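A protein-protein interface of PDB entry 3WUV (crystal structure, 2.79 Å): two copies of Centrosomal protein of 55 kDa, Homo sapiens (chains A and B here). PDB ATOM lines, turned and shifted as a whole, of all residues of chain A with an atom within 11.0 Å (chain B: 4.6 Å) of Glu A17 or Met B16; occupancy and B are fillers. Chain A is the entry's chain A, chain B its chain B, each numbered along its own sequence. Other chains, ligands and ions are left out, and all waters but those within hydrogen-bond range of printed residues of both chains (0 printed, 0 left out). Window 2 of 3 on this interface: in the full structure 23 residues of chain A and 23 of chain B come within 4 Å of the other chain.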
ATOM      1  N   SER A   8      19.925  14.681   7.463  1.00  0.00           N
ATOM      2  CA  SER A   8      19.107  14.619   8.640  1.00  0.00           C
ATOM      3  C   SER A   8      18.433  13.281   8.640  1.00  0.00           C
ATOM      4  O   SER A   8      18.244  12.669   9.659  1.00  0.00           O
ATOM      5  CB  SER A   8      18.071  15.708   8.605  1.00  0.00           C
ATOM      6  OG  SER A   8      16.931  15.224   7.957  1.00  0.00           O
ATOM      7  N   SER A   9      18.036  12.822   7.484  1.00  0.00           N
ATOM      8  CA  SER A   9      17.365  11.558   7.446  1.00  0.00           C
ATOM      9  C   SER A   9      18.274  10.463   7.929  1.00  0.00           C
ATOM     10  O   SER A   9      17.834   9.534   8.548  1.00  0.00           O
ATOM     11  CB  SER A   9      16.854  11.275   6.059  1.00  0.00           C
ATOM     12  OG  SER A   9      15.896  12.240   5.721  1.00  0.00           O
ATOM     13  N   ILE A  10      19.543  10.553   7.604  1.00  0.00           N
ATOM     14  CA  ILE A  10      20.499   9.517   7.983  1.00  0.00           C
ATOM     15  C   ILE A  10      20.666   9.474   9.499  1.00  0.00           C
ATOM     16  O   ILE A  10      20.601   8.406  10.110  1.00  0.00           O
ATOM     17  CB  ILE A  10      21.871   9.747   7.324  1.00  0.00           C
ATOM     18  CG1 ILE A  10      21.743   9.674   5.803  1.00  0.00           C
ATOM     19  CG2 ILE A  10      22.884   8.726   7.820  1.00  0.00           C
ATOM     20  CD1 ILE A  10      23.028   9.960   5.066  1.00  0.00           C
ATOM     21  N   ASN A  11      20.884  10.644  10.092  1.00  0.00           N
ATOM     22  CA  ASN A  11      20.945  10.785  11.542  1.00  0.00           C
ATOM     23  C   ASN A  11      19.696  10.224  12.200  1.00  0.00           C
ATOM     24  O   ASN A  11      19.764   9.543  13.223  1.00  0.00           O
ATOM     25  CB  ASN A  11      21.085  12.258  11.919  1.00  0.00           C
ATOM     26  CG  ASN A  11      22.470  12.603  12.417  1.00  0.00           C
ATOM     27  OD1 ASN A  11      23.202  11.741  12.901  1.00  0.00           O
ATOM     28  ND2 ASN A  11      22.834  13.876  12.310  1.00  0.00           N
ATOM     29  N   ASN A  12      18.553  10.520  11.594  1.00  0.00           N
ATOM     30  CA  ASN A  12      17.266  10.071  12.098  1.00  0.00           C
ATOM     31  C   ASN A  12      17.173   8.549  12.128  1.00  0.00           C
ATOM     32  O   ASN A  12      16.499   7.975  12.982  1.00  0.00           O
ATOM     33  CB  ASN A  12      16.145  10.650  11.242  1.00  0.00           C
ATOM     34  CG  ASN A  12      14.805  10.598  11.930  1.00  0.00           C
ATOM     35  OD1 ASN A  12      14.718  10.663  13.157  1.00  0.00           O
ATOM     36  ND2 ASN A  12      13.746  10.480  11.145  1.00  0.00           N
ATOM     37  N   ILE A  13      17.858   7.903  11.190  1.00  0.00           N
ATOM     38  CA  ILE A  13      17.935   6.448  11.158  1.00  0.00           C
ATOM     39  C   ILE A  13      18.905   5.956  12.230  1.00  0.00           C
ATOM     40  O   ILE A  13      18.720   4.881  12.806  1.00  0.00           O
ATOM     41  CB  ILE A  13      18.368   5.935   9.768  1.00  0.00           C
ATOM     42  CG1 ILE A  13      17.353   6.358   8.708  1.00  0.00           C
ATOM     43  CG2 ILE A  13      18.487   4.425   9.759  1.00  0.00           C
ATOM     44  CD1 ILE A  13      15.969   5.813   8.956  1.00  0.00           C
ATOM     45  N   HIS A  14      19.930   6.755  12.506  1.00  0.00           N
ATOM     46  CA  HIS A  14      20.907   6.413  13.535  1.00  0.00           C
ATOM     47  C   HIS A  14      20.271   6.436  14.921  1.00  0.00           C
ATOM     48  O   HIS A  14      20.564   5.585  15.760  1.00  0.00           O
ATOM     49  CB  HIS A  14      22.104   7.366  13.486  1.00  0.00           C
ATOM     50  CG  HIS A  14      23.202   7.009  14.435  1.00  0.00           C
ATOM     51  ND1 HIS A  14      23.759   5.746  14.493  1.00  0.00           N
ATOM     52  CD2 HIS A  14      23.856   7.744  15.365  1.00  0.00           C
ATOM     53  CE1 HIS A  14      24.701   5.723  15.414  1.00  0.00           C
ATOM     54  NE2 HIS A  14      24.782   6.925  15.961  1.00  0.00           N
ATOM     55  N   GLU A  15      19.398   7.413  15.156  1.00  0.00           N
ATOM     56  CA  GLU A  15      18.660   7.493  16.411  1.00  0.00           C
ATOM     57  C   GLU A  15      17.766   6.275  16.562  1.00  0.00           C
ATOM     58  O   GLU A  15      17.623   5.724  17.650  1.00  0.00           O
ATOM     59  CB  GLU A  15      17.809   8.763  16.460  1.00  0.00           C
ATOM     60  CG  GLU A  15      18.619  10.043  16.481  1.00  0.00           C
ATOM     61  CD  GLU A  15      19.582  10.099  17.651  1.00  0.00           C
ATOM     62  OE1 GLU A  15      19.203   9.660  18.759  1.00  0.00           O
ATOM     63  OE2 GLU A  15      20.721  10.576  17.461  1.00  0.00           O
ATOM     64  N   MET A  16      17.170   5.864  15.451  1.00  0.00           N
ATOM     65  CA  MET A  16      16.310   4.694  15.419  1.00  0.00           C
ATOM     66  C   MET A  16      17.082   3.450  15.840  1.00  0.00           C
ATOM     67  O   MET A  16      16.563   2.594  16.557  1.00  0.00           O
ATOM     68  CB  MET A  16      15.752   4.517  14.011  1.00  0.00           C
ATOM     69  CG  MET A  16      14.814   3.350  13.844  1.00  0.00           C
ATOM     70  SD  MET A  16      13.967   3.459  12.263  1.00  0.00           S
ATOM     71  CE  MET A  16      13.094   5.008  12.475  1.00  0.00           C
ATOM     72  N   GLU A  17      18.333   3.366  15.399  1.00  0.00           N
ATOM     73  CA  GLU A  17      19.176   2.217  15.697  1.00  0.00           C
ATOM     74  C   GLU A  17      19.589   2.167  17.165  1.00  0.00           C
ATOM     75  O   GLU A  17      19.576   1.100  17.777  1.00  0.00           O
ATOM     76  CB  GLU A  17      20.412   2.209  14.793  1.00  0.00           C
ATOM     77  CG  GLU A  17      21.253   0.944  14.884  1.00  0.00           C
ATOM     78  CD  GLU A  17      22.364   1.046  15.914  1.00  0.00           C
ATOM     79  OE1 GLU A  17      22.473   2.101  16.573  1.00  0.00           O
ATOM     80  OE2 GLU A  17      23.130   0.073  16.063  1.00  0.00           O
ATOM     81  N   ILE A  18      19.969   3.309  17.731  1.00  0.00           N
ATOM     82  CA  ILE A  18      20.357   3.334  19.138  1.00  0.00           C
ATOM     83  C   ILE A  18      19.131   3.138  20.027  1.00  0.00           C
ATOM     84  O   ILE A  18      19.232   2.615  21.137  1.00  0.00           O
ATOM     85  CB  ILE A  18      21.119   4.627  19.532  1.00  0.00           C
ATOM     86  CG1 ILE A  18      20.202   5.850  19.483  1.00  0.00           C
ATOM     87  CG2 ILE A  18      22.337   4.827  18.641  1.00  0.00           C
ATOM     88  CD1 ILE A  18      20.847   7.113  20.009  1.00  0.00           C
ATOM     89  N   GLN A  19      17.973   3.546  19.518  1.00  0.00           N
ATOM     90  CA  GLN A  19      16.708   3.377  20.221  1.00  0.00           C
ATOM     91  C   GLN A  19      16.318   1.901  20.248  1.00  0.00           C
ATOM     92  O   GLN A  19      15.730   1.421  21.216  1.00  0.00           O
ATOM     93  CB  GLN A  19      15.618   4.205  19.539  1.00  0.00           C
ATOM     94  CG  GLN A  19      14.258   4.136  20.200  1.00  0.00           C
ATOM     95  CD  GLN A  19      13.233   5.005  19.497  1.00  0.00           C
ATOM     96  OE1 GLN A  19      13.567   5.769  18.592  1.00  0.00           O
ATOM     97  NE2 GLN A  19      11.977   4.892  19.912  1.00  0.00           N
ATOM     98  N   LEU A  20      16.656   1.186  19.180  1.00  0.00           N
ATOM     99  CA  LEU A  20      16.424  -0.253  19.113  1.00  0.00           C
ATOM    100  C   LEU A  20      17.306  -0.988  20.115  1.00  0.00           C
ATOM    101  O   LEU A  20      16.838  -1.856  20.854  1.00  0.00           O
ATOM    102  CB  LEU A  20      16.699  -0.772  17.700  1.00  0.00           C
ATOM    103  CG  LEU A  20      16.751  -2.296  17.566  1.00  0.00           C
ATOM    104  CD1 LEU A  20      15.444  -2.927  18.021  1.00  0.00           C
ATOM    105  CD2 LEU A  20      17.074  -2.709  16.140  1.00  0.00           C
ATOM    106  N   LYS A  21      18.585  -0.628  20.129  1.00  0.00           N
ATOM    107  CA  LYS A  21      19.557  -1.229  21.032  1.00  0.00           C
ATOM    108  C   LYS A  21      19.182  -0.978  22.491  1.00  0.00           C
ATOM    109  O   LYS A  21      19.331  -1.863  23.337  1.00  0.00           O
ATOM    110  CB  LYS A  21      20.944  -0.656  20.752  1.00  0.00           C
ATOM    111  CG  LYS A  21      22.067  -1.354  21.498  1.00  0.00           C
ATOM    112  CD  LYS A  21      23.375  -0.610  21.305  1.00  0.00           C
ATOM    113  CE  LYS A  21      24.517  -1.277  22.050  1.00  0.00           C
ATOM    114  NZ  LYS A  21      25.736  -0.424  22.007  1.00  0.00           N
ATOM    115  N   ASP A  22      18.702   0.230  22.777  1.00  0.00           N
ATOM    116  CA  ASP A  22      18.263   0.587  24.122  1.00  0.00           C
ATOM    117  C   ASP A  22      17.106  -0.296  24.578  1.00  0.00           C
ATOM    118  O   ASP A  22      17.152  -0.881  25.661  1.00  0.00           O
ATOM    119  CB  ASP A  22      17.851   2.059  24.166  1.00  0.00           C
ATOM    120  CG  ASP A  22      17.294   2.474  25.519  1.00  0.00           C
ATOM    121  OD1 ASP A  22      18.090   2.622  26.474  1.00  0.00           O
ATOM    122  OD2 ASP A  22      16.062   2.662  25.627  1.00  0.00           O
ATOM    123  N   ALA A  23      16.077  -0.383  23.741  1.00  0.00           N
ATOM    124  CA  ALA A  23      14.890  -1.178  24.044  1.00  0.00           C
ATOM    125  C   ALA A  23      15.229  -2.648  24.277  1.00  0.00           C
ATOM    126  O   ALA A  23      14.705  -3.274  25.197  1.00  0.00           O
ATOM    127  CB  ALA A  23      13.868  -1.039  22.927  1.00  0.00           C
ATOM    128  N   LEU A  24      16.104  -3.190  23.437  1.00  0.00           N
ATOM    129  CA  LEU A  24      16.547  -4.575  23.564  1.00  0.00           C
ATOM    130  C   LEU A  24      17.295  -4.815  24.874  1.00  0.00           C
ATOM    131  O   LEU A  24      17.224  -5.904  25.447  1.00  0.00           O
ATOM    132  CB  LEU A  24      17.429  -4.956  22.374  1.00  0.00           C
ATOM    133  CG  LEU A  24      16.808  -5.820  21.274  1.00  0.00           C
ATOM    134  CD1 LEU A  24      15.313  -5.591  21.173  1.00  0.00           C
ATOM    135  CD2 LEU A  24      17.478  -5.530  19.944  1.00  0.00           C
ATOM    136  N   GLU A  25      18.014  -3.800  25.338  1.00  0.00           N
ATOM    137  CA  GLU A  25      18.714  -3.884  26.615  1.00  0.00           C
ATOM    138  C   GLU A  25      17.726  -3.874  27.774  1.00  0.00           C
ATOM    139  O   GLU A  25      17.798  -4.712  28.672  1.00  0.00           O
ATOM    140  CB  GLU A  25      19.696  -2.722  26.774  1.00  0.00           C
ATOM    141  CG  GLU A  25      21.076  -2.979  26.199  1.00  0.00           C
ATOM    142  CD  GLU A  25      22.020  -1.813  26.425  1.00  0.00           C
ATOM    143  OE1 GLU A  25      23.154  -1.853  25.901  1.00  0.00           O
ATOM    144  OE2 GLU A  25      21.626  -0.856  27.125  1.00  0.00           O
ATOM    145  N   ASN B  12      17.237  -3.646   5.128  1.00  0.00           N
ATOM    146  CA  ASN B  12      17.791  -3.988   6.431  1.00  0.00           C
ATOM    147  C   ASN B  12      17.368  -2.888   7.399  1.00  0.00           C
ATOM    148  O   ASN B  12      16.978  -3.156   8.535  1.00  0.00           O
ATOM    149  CB  ASN B  12      19.315  -4.119   6.370  1.00  0.00           C
ATOM    150  CG  ASN B  12      19.828  -5.355   7.103  1.00  0.00           C
ATOM    151  OD1 ASN B  12      19.102  -6.332   7.289  1.00  0.00           O
ATOM    152  ND2 ASN B  12      21.089  -5.314   7.516  1.00  0.00           N
ATOM    153  N   ILE B  13      17.413  -1.649   6.916  1.00  0.00           N
ATOM    154  CA  ILE B  13      16.855  -0.511   7.638  1.00  0.00           C
ATOM    155  C   ILE B  13      15.351  -0.689   7.854  1.00  0.00           C
ATOM    156  O   ILE B  13      14.837  -0.391   8.933  1.00  0.00           O
ATOM    157  CB  ILE B  13      17.114   0.817   6.892  1.00  0.00           C
ATOM    158  CG1 ILE B  13      18.614   1.048   6.717  1.00  0.00           C
ATOM    159  CG2 ILE B  13      16.477   1.986   7.627  1.00  0.00           C
ATOM    160  CD1 ILE B  13      19.391   0.939   7.999  1.00  0.00           C
ATOM    161  N   HIS B  14      14.648  -1.174   6.832  1.00  0.00           N
ATOM    162  CA  HIS B  14      13.214  -1.437   6.957  1.00  0.00           C
ATOM    163  C   HIS B  14      12.965  -2.488   8.032  1.00  0.00           C
ATOM    164  O   HIS B  14      12.061  -2.347   8.854  1.00  0.00           O
ATOM    165  CB  HIS B  14      12.616  -1.892   5.621  1.00  0.00           C
ATOM    166  CG  HIS B  14      11.127  -2.044   5.643  1.00  0.00           C
ATOM    167  ND1 HIS B  14      10.488  -3.208   5.265  1.00  0.00           N
ATOM    168  CD2 HIS B  14      10.147  -1.179   5.995  1.00  0.00           C
ATOM    169  CE1 HIS B  14       9.183  -3.051   5.384  1.00  0.00           C
ATOM    170  NE2 HIS B  14       8.949  -1.827   5.827  1.00  0.00           N
ATOM    171  N   GLU B  15      13.782  -3.537   8.023  1.00  0.00           N
ATOM    172  CA  GLU B  15      13.702  -4.582   9.036  1.00  0.00           C
ATOM    173  C   GLU B  15      14.047  -4.042  10.420  1.00  0.00           C
ATOM    174  O   GLU B  15      13.460  -4.456  11.420  1.00  0.00           O
ATOM    175  CB  GLU B  15      14.646  -5.739   8.693  1.00  0.00           C
ATOM    176  CG  GLU B  15      13.946  -7.024   8.270  1.00  0.00           C
ATOM    177  CD  GLU B  15      13.346  -7.799   9.436  1.00  0.00           C
ATOM    178  OE1 GLU B  15      12.969  -8.973   9.232  1.00  0.00           O
ATOM    179  OE2 GLU B  15      13.249  -7.245  10.552  1.00  0.00           O
ATOM    180  N   MET B  16      15.001  -3.117  10.471  1.00  0.00           N
ATOM    181  CA  MET B  16      15.483  -2.571  11.738  1.00  0.00           C
ATOM    182  C   MET B  16      14.373  -1.856  12.502  1.00  0.00           C
ATOM    183  O   MET B  16      14.353  -1.838  13.734  1.00  0.00           O
ATOM    184  CB  MET B  16      16.652  -1.613  11.497  1.00  0.00           C
ATOM    185  CG  MET B  16      17.428  -1.283  12.758  1.00  0.00           C
ATOM    186  SD  MET B  16      18.616   0.054  12.547  1.00  0.00           S
ATOM    187  CE  MET B  16      17.518   1.447  12.307  1.00  0.00           C
ATOM    188  N   GLU B  17      13.441  -1.290  11.741  1.00  0.00           N
ATOM    189  CA  GLU B  17      12.327  -0.510  12.263  1.00  0.00           C
ATOM    190  C   GLU B  17      11.097  -1.408  12.443  1.00  0.00           C
ATOM    191  O   GLU B  17      10.109  -1.010  13.067  1.00  0.00           O
ATOM    192  CB  GLU B  17      12.061   0.658  11.306  1.00  0.00           C
ATOM    193  CG  GLU B  17      10.733   1.383  11.426  1.00  0.00           C
ATOM    194  CD  GLU B  17      10.196   1.804  10.070  1.00  0.00           C
ATOM    195  OE1 GLU B  17      10.599   1.201   9.053  1.00  0.00           O
ATOM    196  OE2 GLU B  17       9.370   2.735  10.022  1.00  0.00           O
ATOM    197  N   ILE B  18      11.163  -2.623  11.903  1.00  0.00           N
ATOM    198  CA  ILE B  18      10.243  -3.675  12.324  1.00  0.00           C
ATOM    199  C   ILE B  18      10.667  -4.141  13.713  1.00  0.00           C
ATOM    200  O   ILE B  18       9.906  -4.030  14.673  1.00  0.00           O
ATOM    201  CB  ILE B  18      10.234  -4.894  11.371  1.00  0.00           C
ATOM    202  CG1 ILE B  18       9.712  -4.501   9.984  1.00  0.00           C
ATOM    203  CG2 ILE B  18       9.404  -6.039  11.967  1.00  0.00           C
ATOM    204  CD1 ILE B  18       9.032  -5.632   9.230  1.00  0.00           C
ATOM    205  N   GLN B  19      11.895  -4.649  13.805  1.00  0.00           N
ATOM    206  CA  GLN B  19      12.456  -5.135  15.066  1.00  0.00           C
ATOM    207  C   GLN B  19      12.380  -4.091  16.181  1.00  0.00           C
ATOM    208  O   GLN B  19      12.221  -4.437  17.351  1.00  0.00           O
ATOM    209  CB  GLN B  19      13.903  -5.603  14.873  1.00  0.00           C
ATOM    210  CG  GLN B  19      14.050  -6.814  13.963  1.00  0.00           C
ATOM    211  CD  GLN B  19      15.487  -7.283  13.831  1.00  0.00           C
ATOM    212  OE1 GLN B  19      16.385  -6.770  14.500  1.00  0.00           O
ATOM    213  NE2 GLN B  19      15.712  -8.262  12.964  1.00  0.00           N
ATOM    214  N   LEU B  20      12.491  -2.818  15.811  1.00  0.00           N
ATOM    215  CA  LEU B  20      12.328  -1.731  16.769  1.00  0.00           C
ATOM    216  C   LEU B  20      10.894  -1.667  17.272  1.00  0.00           C
ATOM    217  O   LEU B  20      10.644  -1.675  18.478  1.00  0.00           O
ATOM    218  CB  LEU B  20      12.703  -0.390  16.142  1.00  0.00           C
ATOM    219  CG  LEU B  20      12.298   0.814  16.996  1.00  0.00           C
ATOM    220  CD1 LEU B  20      13.083   0.843  18.298  1.00  0.00           C
ATOM    221  CD2 LEU B  20      12.469   2.113  16.235  1.00  0.00           C
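Among the printed residues, pairs that only touch across the chains: Met A16 with Glu B17 (3.5 Å), Leu A20 with Leu B20 (3.6 Å), Met A16 with Leu B20 (3.6 Å), Glu A17 with Met B16 (3.6 Å), Leu A20 with Gln B19 (3.6 Å), Met A16 with Met B16 (3.6 Å), Ile A13 with Met B16 (3.7 Å), Leu A20 with Met B16 (3.7 Å), Ile A13 with Ile B13 (3.8 Å) and Gln A19 with Leu B20 (3.9 Å).
Glu A17 touches just one residue of chain B: Met B16. No residue of chain A comes within 4 Å of Glu B15. No residue of chain A comes within 4 Å of Ile B18. Leu B20 touches three residues of chain A. Of the printed residues of chain A, Glu B17 touches Met A16 (3.5 Å). Of the printed residues of chain B, Ile A13 touches Ile B13 and Met B16. Of the printed residues of chain B, Gln A19 touches Leu B20. Printed residues of chain B within 4 Å of Met A16: Met B16, Glu B17 and Leu B20. Of the printed residues of chain B, Leu A20 touches Met B16 (3.7 Å), Gln B19 (3.6 Å) and Leu B20 (3.6 Å). Ser A8 touches none of the printed residues of chain B. Asn A12 touches none of the printed residues of chain B. The nearest printed residue of chain B that does not touch Glu A17 is Leu B20 (6.1 Å). The nearest residue of chain A that does not touch Met B16 is His A14 (5.8 Å).
Hydrophobic or aromatic side chains of chain A within 4 Å of the printed part of chain B: Ile A13, Met A16 and Leu A20. Of the 9 printed residues of chain B, 5 touch a printed residue of chain A. Hydrophobic or aromatic side chains of chain B within 4 Å of the printed part of chain A: Ile B13, Met B16 and Leu B20. Among the printed residues, no Asp or Glu carboxylate lies within 4 Å of a Lys or Arg side-chain nitrogen of the other chain.
Ile B13 touches its own counterpart, Ile A13. Met A16 touches Leu B20, and with the chains exchanged Leu A20 touches Met B16. Gln A19 touches Leu B20, and with the chains exchanged Leu A20 touches Gln B19. Leu B20 touches its own counterpart, Leu A20. Positions printed for both chains: 12, 13, 14, 15, 16, 17, 18, 19 and 20.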
